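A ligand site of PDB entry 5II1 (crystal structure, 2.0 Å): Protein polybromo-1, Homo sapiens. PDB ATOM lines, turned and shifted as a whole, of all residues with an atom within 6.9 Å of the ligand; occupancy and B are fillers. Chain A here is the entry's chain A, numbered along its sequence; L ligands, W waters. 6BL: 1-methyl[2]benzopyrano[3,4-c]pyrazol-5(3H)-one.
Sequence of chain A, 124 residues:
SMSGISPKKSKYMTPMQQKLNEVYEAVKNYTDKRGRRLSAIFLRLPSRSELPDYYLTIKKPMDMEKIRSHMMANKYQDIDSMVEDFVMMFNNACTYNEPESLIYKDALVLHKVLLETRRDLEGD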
ATOM      1  N   ALA A  40      29.158 -22.269 -15.575  1.00  0.00           N
ATOM      2  CA  ALA A  40      28.069 -23.272 -15.715  1.00  0.00           C
ATOM      3  C   ALA A  40      26.852 -22.899 -14.889  1.00  0.00           C
ATOM      4  O   ALA A  40      25.792 -22.717 -15.436  1.00  0.00           O
ATOM      5  CB  ALA A  40      28.540 -24.655 -15.299  1.00  0.00           C
ATOM      6  N   ILE A  41      27.066 -22.731 -13.596  1.00  0.00           N
ATOM      7  CA  ILE A  41      25.982 -22.489 -12.666  1.00  0.00           C
ATOM      8  C   ILE A  41      25.367 -21.085 -12.818  1.00  0.00           C
ATOM      9  O   ILE A  41      24.257 -20.849 -12.347  1.00  0.00           O
ATOM     10  CB  ILE A  41      26.441 -22.781 -11.199  1.00  0.00           C
ATOM     11  CG1 ILE A  41      25.244 -23.091 -10.267  1.00  0.00           C
ATOM     12  CG2 ILE A  41      27.218 -21.654 -10.593  1.00  0.00           C
ATOM     13  CD1 ILE A  41      24.505 -24.373 -10.597  1.00  0.00           C
ATOM     14  N   PHE A  42      26.087 -20.150 -13.469  1.00  0.00           N
ATOM     15  CA  PHE A  42      25.696 -18.753 -13.616  1.00  0.00           C
ATOM     16  C   PHE A  42      24.852 -18.461 -14.858  1.00  0.00           C
ATOM     17  O   PHE A  42      24.278 -17.365 -14.968  1.00  0.00           O
ATOM     18  CB  PHE A  42      26.956 -17.846 -13.596  1.00  0.00           C
ATOM     19  CG  PHE A  42      27.672 -17.842 -12.249  1.00  0.00           C
ATOM     20  CD1 PHE A  42      27.151 -17.146 -11.156  1.00  0.00           C
ATOM     21  CD2 PHE A  42      28.847 -18.574 -12.062  1.00  0.00           C
ATOM     22  CE1 PHE A  42      27.810 -17.174  -9.929  1.00  0.00           C
ATOM     23  CE2 PHE A  42      29.507 -18.602 -10.836  1.00  0.00           C
ATOM     24  CZ  PHE A  42      28.996 -17.908  -9.774  1.00  0.00           C
ATOM     25  N   LEU A  43      24.760 -19.425 -15.795  1.00  0.00           N
ATOM     26  CA  LEU A  43      24.079 -19.190 -17.096  1.00  0.00           C
ATOM     27  C   LEU A  43      22.595 -18.817 -16.899  1.00  0.00           C
ATOM     28  O   LEU A  43      22.140 -17.805 -17.397  1.00  0.00           O
ATOM     29  CB  LEU A  43      24.223 -20.386 -18.038  1.00  0.00           C
ATOM     30  CG  LEU A  43      25.673 -20.780 -18.435  1.00  0.00           C
ATOM     31  CD1 LEU A  43      25.708 -21.889 -19.487  1.00  0.00           C
ATOM     32  CD2 LEU A  43      26.507 -19.582 -18.869  1.00  0.00           C
ATOM     33  N   ARG A  44      21.876 -19.600 -16.092  1.00  0.00           N
ATOM     34  CA  ARG A  44      20.446 -19.383 -15.865  1.00  0.00           C
ATOM     35  C   ARG A  44      20.067 -19.606 -14.399  1.00  0.00           C
ATOM     36  O   ARG A  44      20.262 -20.683 -13.860  1.00  0.00           O
ATOM     37  CB  ARG A  44      19.633 -20.306 -16.761  1.00  0.00           C
ATOM     38  CG  ARG A  44      18.154 -20.044 -16.756  1.00  0.00           C
ATOM     39  CD  ARG A  44      17.836 -18.861 -17.602  1.00  0.00           C
ATOM     40  NE  ARG A  44      16.407 -18.672 -17.652  1.00  0.00           N
ATOM     41  CZ  ARG A  44      15.699 -18.011 -16.738  1.00  0.00           C
ATOM     42  NH1 ARG A  44      14.372 -17.910 -16.889  1.00  0.00           N
ATOM     43  NH2 ARG A  44      16.286 -17.460 -15.656  1.00  0.00           N
ATOM     44  N   LEU A  45      19.528 -18.564 -13.778  1.00  0.00           N
ATOM     45  CA  LEU A  45      18.954 -18.656 -12.443  1.00  0.00           C
ATOM     46  C   LEU A  45      17.819 -19.676 -12.413  1.00  0.00           C
ATOM     47  O   LEU A  45      16.989 -19.723 -13.312  1.00  0.00           O
ATOM     48  CB  LEU A  45      18.351 -17.338 -11.996  1.00  0.00           C
ATOM     49  CG  LEU A  45      19.245 -16.395 -11.227  1.00  0.00           C
ATOM     50  CD1 LEU A  45      18.551 -15.047 -11.211  1.00  0.00           C
ATOM     51  CD2 LEU A  45      19.515 -16.882  -9.806  1.00  0.00           C
ATOM     52  N   PRO A  46      17.759 -20.453 -11.333  1.00  0.00           N
ATOM     53  CA  PRO A  46      16.553 -21.193 -11.060  1.00  0.00           C
ATOM     54  C   PRO A  46      15.309 -20.302 -10.812  1.00  0.00           C
ATOM     55  O   PRO A  46      15.399 -19.087 -10.602  1.00  0.00           O
ATOM     56  CB  PRO A  46      16.908 -21.969  -9.784  1.00  0.00           C
ATOM     57  CG  PRO A  46      18.397 -21.980  -9.754  1.00  0.00           C
ATOM     58  CD  PRO A  46      18.755 -20.652 -10.276  1.00  0.00           C
ATOM     59  N   LEU A  51      14.458 -21.649  -5.887  1.00  0.00           N
ATOM     60  CA  LEU A  51      15.484 -20.945  -5.102  1.00  0.00           C
ATOM     61  C   LEU A  51      14.805 -19.714  -4.433  1.00  0.00           C
ATOM     62  O   LEU A  51      15.266 -18.597  -4.604  1.00  0.00           O
ATOM     63  CB  LEU A  51      16.676 -20.548  -6.012  1.00  0.00           C
ATOM     64  CG  LEU A  51      18.044 -20.288  -5.384  1.00  0.00           C
ATOM     65  CD1 LEU A  51      18.696 -21.569  -4.885  1.00  0.00           C
ATOM     66  CD2 LEU A  51      18.969 -19.588  -6.367  1.00  0.00           C
ATOM     67  N   TYR A  54      16.980 -16.962  -2.434  1.00  0.00           N
ATOM     68  CA  TYR A  54      17.694 -16.021  -3.284  1.00  0.00           C
ATOM     69  C   TYR A  54      16.793 -14.806  -3.555  1.00  0.00           C
ATOM     70  O   TYR A  54      17.191 -13.663  -3.339  1.00  0.00           O
ATOM     71  CB  TYR A  54      18.147 -16.694  -4.594  1.00  0.00           C
ATOM     72  CG  TYR A  54      18.729 -15.744  -5.617  1.00  0.00           C
ATOM     73  CD1 TYR A  54      17.899 -15.043  -6.490  1.00  0.00           C
ATOM     74  CD2 TYR A  54      20.135 -15.549  -5.741  1.00  0.00           C
ATOM     75  CE1 TYR A  54      18.413 -14.178  -7.435  1.00  0.00           C
ATOM     76  CE2 TYR A  54      20.669 -14.670  -6.687  1.00  0.00           C
ATOM     77  CZ  TYR A  54      19.794 -13.988  -7.538  1.00  0.00           C
ATOM     78  OH  TYR A  54      20.254 -13.152  -8.480  1.00  0.00           O
ATOM     79  N   ILE A  58      17.723 -10.930  -2.506  1.00  0.00           N
ATOM     80  CA  ILE A  58      18.425 -10.228  -3.602  1.00  0.00           C
ATOM     81  C   ILE A  58      17.457  -9.290  -4.277  1.00  0.00           C
ATOM     82  O   ILE A  58      16.433  -9.738  -4.776  1.00  0.00           O
ATOM     83  CB  ILE A  58      18.994 -11.262  -4.624  1.00  0.00           C
ATOM     84  CG1 ILE A  58      20.061 -12.137  -3.965  1.00  0.00           C
ATOM     85  CG2 ILE A  58      19.518 -10.570  -5.872  1.00  0.00           C
ATOM     86  CD1 ILE A  58      21.261 -11.398  -3.355  1.00  0.00           C
ATOM     87  N   MET A  62      20.040 -11.545 -11.343  1.00  0.00           N
ATOM     88  CA  MET A  62      20.867 -11.446 -12.555  1.00  0.00           C
ATOM     89  C   MET A  62      21.436 -12.807 -12.868  1.00  0.00           C
ATOM     90  O   MET A  62      21.825 -13.536 -11.932  1.00  0.00           O
ATOM     91  CB  MET A  62      22.012 -10.432 -12.316  1.00  0.00           C
ATOM     92  CG  MET A  62      22.784 -10.041 -13.576  1.00  0.00           C
ATOM     93  SD  MET A  62      21.788  -9.450 -14.940  1.00  0.00           S
ATOM     94  CE  MET A  62      21.046  -7.961 -14.247  1.00  0.00           C
ATOM     95  N   ASP A  63      21.433 -13.164 -14.160  1.00  0.00           N
ATOM     96  CA  ASP A  63      22.123 -14.323 -14.653  1.00  0.00           C
ATOM     97  C   ASP A  63      22.739 -13.994 -16.042  1.00  0.00           C
ATOM     98  O   ASP A  63      22.523 -12.891 -16.568  1.00  0.00           O
ATOM     99  CB  ASP A  63      21.227 -15.576 -14.651  1.00  0.00           C
ATOM    100  CG  ASP A  63      19.976 -15.473 -15.543  1.00  0.00           C
ATOM    101  OD1 ASP A  63      19.923 -14.656 -16.474  1.00  0.00           O
ATOM    102  OD2 ASP A  63      19.051 -16.272 -15.347  1.00  0.00           O
ATOM    103  N   MET A  64      23.571 -14.879 -16.569  1.00  0.00           N
ATOM    104  CA  MET A  64      24.307 -14.591 -17.801  1.00  0.00           C
ATOM    105  C   MET A  64      23.425 -14.581 -19.037  1.00  0.00           C
ATOM    106  O   MET A  64      23.696 -13.844 -19.961  1.00  0.00           O
ATOM    107  CB  MET A  64      25.467 -15.551 -17.976  1.00  0.00           C
ATOM    108  CG  MET A  64      26.520 -15.394 -16.891  1.00  0.00           C
ATOM    109  SD  MET A  64      28.062 -16.276 -17.101  1.00  0.00           S
ATOM    110  CE  MET A  64      28.511 -15.807 -18.778  1.00  0.00           C
ATOM    111  N   MET A  88      27.230  -7.100 -10.426  1.00  0.00           N
ATOM    112  CA  MET A  88      25.996  -7.288  -9.676  1.00  0.00           C
ATOM    113  C   MET A  88      25.694  -8.779  -9.474  1.00  0.00           C
ATOM    114  O   MET A  88      25.359  -9.226  -8.361  1.00  0.00           O
ATOM    115  CB  MET A  88      24.860  -6.576 -10.422  1.00  0.00           C
ATOM    116  CG  MET A  88      23.416  -7.002 -10.160  1.00  0.00           C
ATOM    117  SD  MET A  88      22.486  -5.914  -9.115  1.00  0.00           S
ATOM    118  CE  MET A  88      23.420  -6.123  -7.630  1.00  0.00           C
ATOM    119  N   MET A  89      25.828  -9.546 -10.567  1.00  0.00           N
ATOM    120  CA  MET A  89      25.645 -10.985 -10.511  1.00  0.00           C
ATOM    121  C   MET A  89      26.567 -11.645  -9.462  1.00  0.00           C
ATOM    122  O   MET A  89      26.112 -12.465  -8.631  1.00  0.00           O
ATOM    123  CB  MET A  89      25.834 -11.625 -11.898  1.00  0.00           C
ATOM    124  CG  MET A  89      25.430 -13.081 -11.947  1.00  0.00           C
ATOM    125  SD  MET A  89      25.639 -13.842 -13.578  1.00  0.00           S
ATOM    126  CE  MET A  89      27.413 -13.959 -13.634  1.00  0.00           C
ATOM    127  N   PHE A  90      27.836 -11.291  -9.484  1.00  0.00           N
ATOM    128  CA  PHE A  90      28.814 -11.939  -8.595  1.00  0.00           C
ATOM    129  C   PHE A  90      28.636 -11.492  -7.148  1.00  0.00           C
ATOM    130  O   PHE A  90      28.774 -12.296  -6.216  1.00  0.00           O
ATOM    131  CB  PHE A  90      30.235 -11.708  -9.101  1.00  0.00           C
ATOM    132  CG  PHE A  90      30.513 -12.360 -10.475  1.00  0.00           C
ATOM    133  CD1 PHE A  90      30.165 -13.699 -10.719  1.00  0.00           C
ATOM    134  CD2 PHE A  90      31.107 -11.636 -11.509  1.00  0.00           C
ATOM    135  CE1 PHE A  90      30.420 -14.290 -11.955  1.00  0.00           C
ATOM    136  CE2 PHE A  90      31.379 -12.229 -12.730  1.00  0.00           C
ATOM    137  CZ  PHE A  90      31.011 -13.560 -12.953  1.00  0.00           C
ATOM    138  N   ASN A  91      28.307 -10.218  -6.981  1.00  0.00           N
ATOM    139  CA  ASN A  91      27.904  -9.698  -5.658  1.00  0.00           C
ATOM    140  C   ASN A  91      26.650 -10.332  -5.093  1.00  0.00           C
ATOM    141  O   ASN A  91      26.573 -10.574  -3.890  1.00  0.00           O
ATOM    142  CB  ASN A  91      27.662  -8.190  -5.738  1.00  0.00           C
ATOM    143  CG  ASN A  91      28.949  -7.414  -5.721  1.00  0.00           C
ATOM    144  OD1 ASN A  91      29.997  -7.902  -5.301  1.00  0.00           O
ATOM    145  ND2 ASN A  91      28.890  -6.194  -6.215  1.00  0.00           N
ATOM    146  N   ASN A  92      25.625 -10.503  -5.930  1.00  0.00           N
ATOM    147  CA  ASN A  92      24.446 -11.253  -5.521  1.00  0.00           C
ATOM    148  C   ASN A  92      24.855 -12.629  -5.024  1.00  0.00           C
ATOM    149  O   ASN A  92      24.421 -13.064  -3.947  1.00  0.00           O
ATOM    150  CB  ASN A  92      23.447 -11.414  -6.680  1.00  0.00           C
ATOM    151  CG  ASN A  92      22.695 -10.131  -7.021  1.00  0.00           C
ATOM    152  OD1 ASN A  92      22.734  -9.153  -6.298  1.00  0.00           O
ATOM    153  ND2 ASN A  92      22.074 -10.127  -8.192  1.00  0.00           N
ATOM    154  N   ALA A  93      25.691 -13.325  -5.815  1.00  0.00           N
ATOM    155  CA  ALA A  93      26.162 -14.676  -5.478  1.00  0.00           C
ATOM    156  C   ALA A  93      26.902 -14.721  -4.148  1.00  0.00           C
ATOM    157  O   ALA A  93      26.708 -15.612  -3.340  1.00  0.00           O
ATOM    158  CB  ALA A  93      27.082 -15.209  -6.592  1.00  0.00           C
ATOM    159  N   CYS A  94      27.759 -13.730  -3.934  1.00  0.00           N
ATOM    160  CA  CYS A  94      28.575 -13.604  -2.717  1.00  0.00           C
ATOM    161  C   CYS A  94      27.775 -13.038  -1.497  1.00  0.00           C
ATOM    162  O   CYS A  94      28.151 -13.227  -0.355  1.00  0.00           O
ATOM    163  CB  CYS A  94      29.823 -12.754  -3.031  1.00  0.00           C
ATOM    164  SG  CYS A  94      31.019 -13.579  -4.149  1.00  0.00           S
ATOM    165  N   TYR A  96      24.212 -13.847  -1.204  1.00  0.00           N
ATOM    166  CA  TYR A  96      23.323 -14.943  -0.893  1.00  0.00           C
ATOM    167  C   TYR A  96      24.052 -16.151  -0.310  1.00  0.00           C
ATOM    168  O   TYR A  96      23.545 -16.749   0.608  1.00  0.00           O
ATOM    169  CB  TYR A  96      22.485 -15.310  -2.117  1.00  0.00           C
ATOM    170  CG  TYR A  96      21.620 -16.519  -1.911  1.00  0.00           C
ATOM    171  CD1 TYR A  96      20.634 -16.562  -0.884  1.00  0.00           C
ATOM    172  CD2 TYR A  96      21.767 -17.619  -2.719  1.00  0.00           C
ATOM    173  CE1 TYR A  96      19.841 -17.694  -0.682  1.00  0.00           C
ATOM    174  CE2 TYR A  96      20.986 -18.741  -2.523  1.00  0.00           C
ATOM    175  CZ  TYR A  96      20.039 -18.777  -1.519  1.00  0.00           C
ATOM    176  OH  TYR A  96      19.286 -19.900  -1.381  1.00  0.00           O
ATOM    177  N   ASN A  97      25.206 -16.519  -0.864  1.00  0.00           N
ATOM    178  CA  ASN A  97      26.038 -17.618  -0.391  1.00  0.00           C
ATOM    179  C   ASN A  97      27.144 -17.213   0.562  1.00  0.00           C
ATOM    180  O   ASN A  97      27.496 -16.052   0.664  1.00  0.00           O
ATOM    181  CB  ASN A  97      26.644 -18.353  -1.575  1.00  0.00           C
ATOM    182  CG  ASN A  97      25.571 -18.813  -2.536  1.00  0.00           C
ATOM    183  OD1 ASN A  97      25.031 -19.883  -2.380  1.00  0.00           O
ATOM    184  ND2 ASN A  97      25.269 -17.985  -3.551  1.00  0.00           N
ATOM    185  N   ILE A 103      30.331 -21.866  -4.966  1.00  0.00           N
ATOM    186  CA  ILE A 103      29.753 -20.855  -5.831  1.00  0.00           C
ATOM    187  C   ILE A 103      30.300 -19.448  -5.504  1.00  0.00           C
ATOM    188  O   ILE A 103      30.595 -18.693  -6.398  1.00  0.00           O
ATOM    189  CB  ILE A 103      28.208 -20.886  -5.883  1.00  0.00           C
ATOM    190  CG1 ILE A 103      27.686 -19.878  -6.916  1.00  0.00           C
ATOM    191  CG2 ILE A 103      27.600 -20.584  -4.529  1.00  0.00           C
ATOM    192  CD1 ILE A 103      26.222 -20.067  -7.310  1.00  0.00           C
HETATM  193  CAN 6BL L   1      22.133 -21.228  -8.003  1.00  0.00           C
HETATM  194  CAL 6BL L   1      22.573 -19.947  -7.290  1.00  0.00           C
HETATM  195  CAI 6BL L   1      22.869 -18.703  -7.853  1.00  0.00           C
HETATM  196  CAF 6BL L   1      22.932 -18.123  -9.138  1.00  0.00           C
HETATM  197  CAD 6BL L   1      22.579 -18.843 -10.302  1.00  0.00           C
HETATM  198  CAB 6BL L   1      22.625 -18.272 -11.557  1.00  0.00           C
HETATM  199  CAA 6BL L   1      23.004 -16.924 -11.659  1.00  0.00           C
HETATM  200  CAC 6BL L   1      23.351 -16.189 -10.533  1.00  0.00           C
HETATM  201  CAE 6BL L   1      23.307 -16.762  -9.261  1.00  0.00           C
HETATM  202  CAH 6BL L   1      23.633 -16.053  -8.089  1.00  0.00           C
HETATM  203  OAG 6BL L   1      23.964 -14.873  -8.081  1.00  0.00           O
HETATM  204  OAK 6BL L   1      23.610 -16.658  -6.844  1.00  0.00           O
HETATM  205  CAJ 6BL L   1      23.223 -17.965  -6.722  1.00  0.00           C
HETATM  206  NAO 6BL L   1      23.127 -18.754  -5.657  1.00  0.00           N
HETATM  207  NAM 6BL L   1      22.747 -19.879  -5.985  1.00  0.00           N
HETATM  208  O   HOH W   1      21.820 -21.845 -11.709  1.00  0.00           O
HETATM  209  O   HOH W   2      22.739 -21.821  -3.956  1.00  0.00           O
HETATM  210  O   HOH W   3      22.559 -13.069  -9.478  1.00  0.00           O
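The side-chain amide nitrogen (ND2) of Asn 97 sits close to a nitrogen (NAO) of the ligand (3.1 Å).
OAG of the ligand sits at hydrogen-bond distance from N of Ala 93 (3.2 Å).
The backbone NH (N) of Met 64 lies close to the side-chain sulfur (SD) of Met 89 (3.8 Å).
The backbone carbonyl oxygen (O) of Met 88 lies close to the side-chain amide oxygen (OD1) of Asn 92 (3.3 Å).
The guanidinium group (NH2) of Arg 44 is in salt-bridge range of the side-chain carboxylate (OD2) of Asp 63 (3.0 Å).
The backbone carbonyl oxygen (O) of Phe 42 sits at hydrogen-bond distance from the backbone NH (N) of Met 64.
The backbone carbonyl oxygen of Ala 93 sits at hydrogen-bond distance from the side-chain amide nitrogen of Asn 97 (2.8 Å).
OD2 of Asp 63 sits at hydrogen-bond distance from N of Leu 45 (2.8 Å).
The backbone NH of Met 62 sits at hydrogen-bond distance from the side-chain hydroxyl of Tyr 54 (3.3 Å).
O of Met 89 lies close to OAG of the ligand (3.3 Å).
Ile 41 touches the ligand.
Phe 42 touches the ligand.
Leu 45 touches the ligand (CD2 to CAD, 3.7 Å).
Leu 51 touches the ligand.
Tyr 54 touches the ligand (CE2 to OAK, 3.6 Å).
Met 62 touches the ligand (O to CAC, 3.4 Å).
Asp 63 touches the ligand.
Asn 92 touches the ligand.
CD2 of Tyr 96 touches NAO of the ligand, 3.4 Å away.
Ile 103 touches the ligand.
Of the 23 residues printed, 13 come within 4 Å of the ligand.
The nearest printed residue that does not touch the ligand is Arg 44 (4.05 Å).
Water W3 lies within hydrogen-bond range of OH of Tyr 54, O of Met 62, OAG of the ligand and ND2 of Asn 92.
Water W2 bridges NAM of the ligand (2.8 Å) and OD1 of Asn 97 (3.4 Å).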
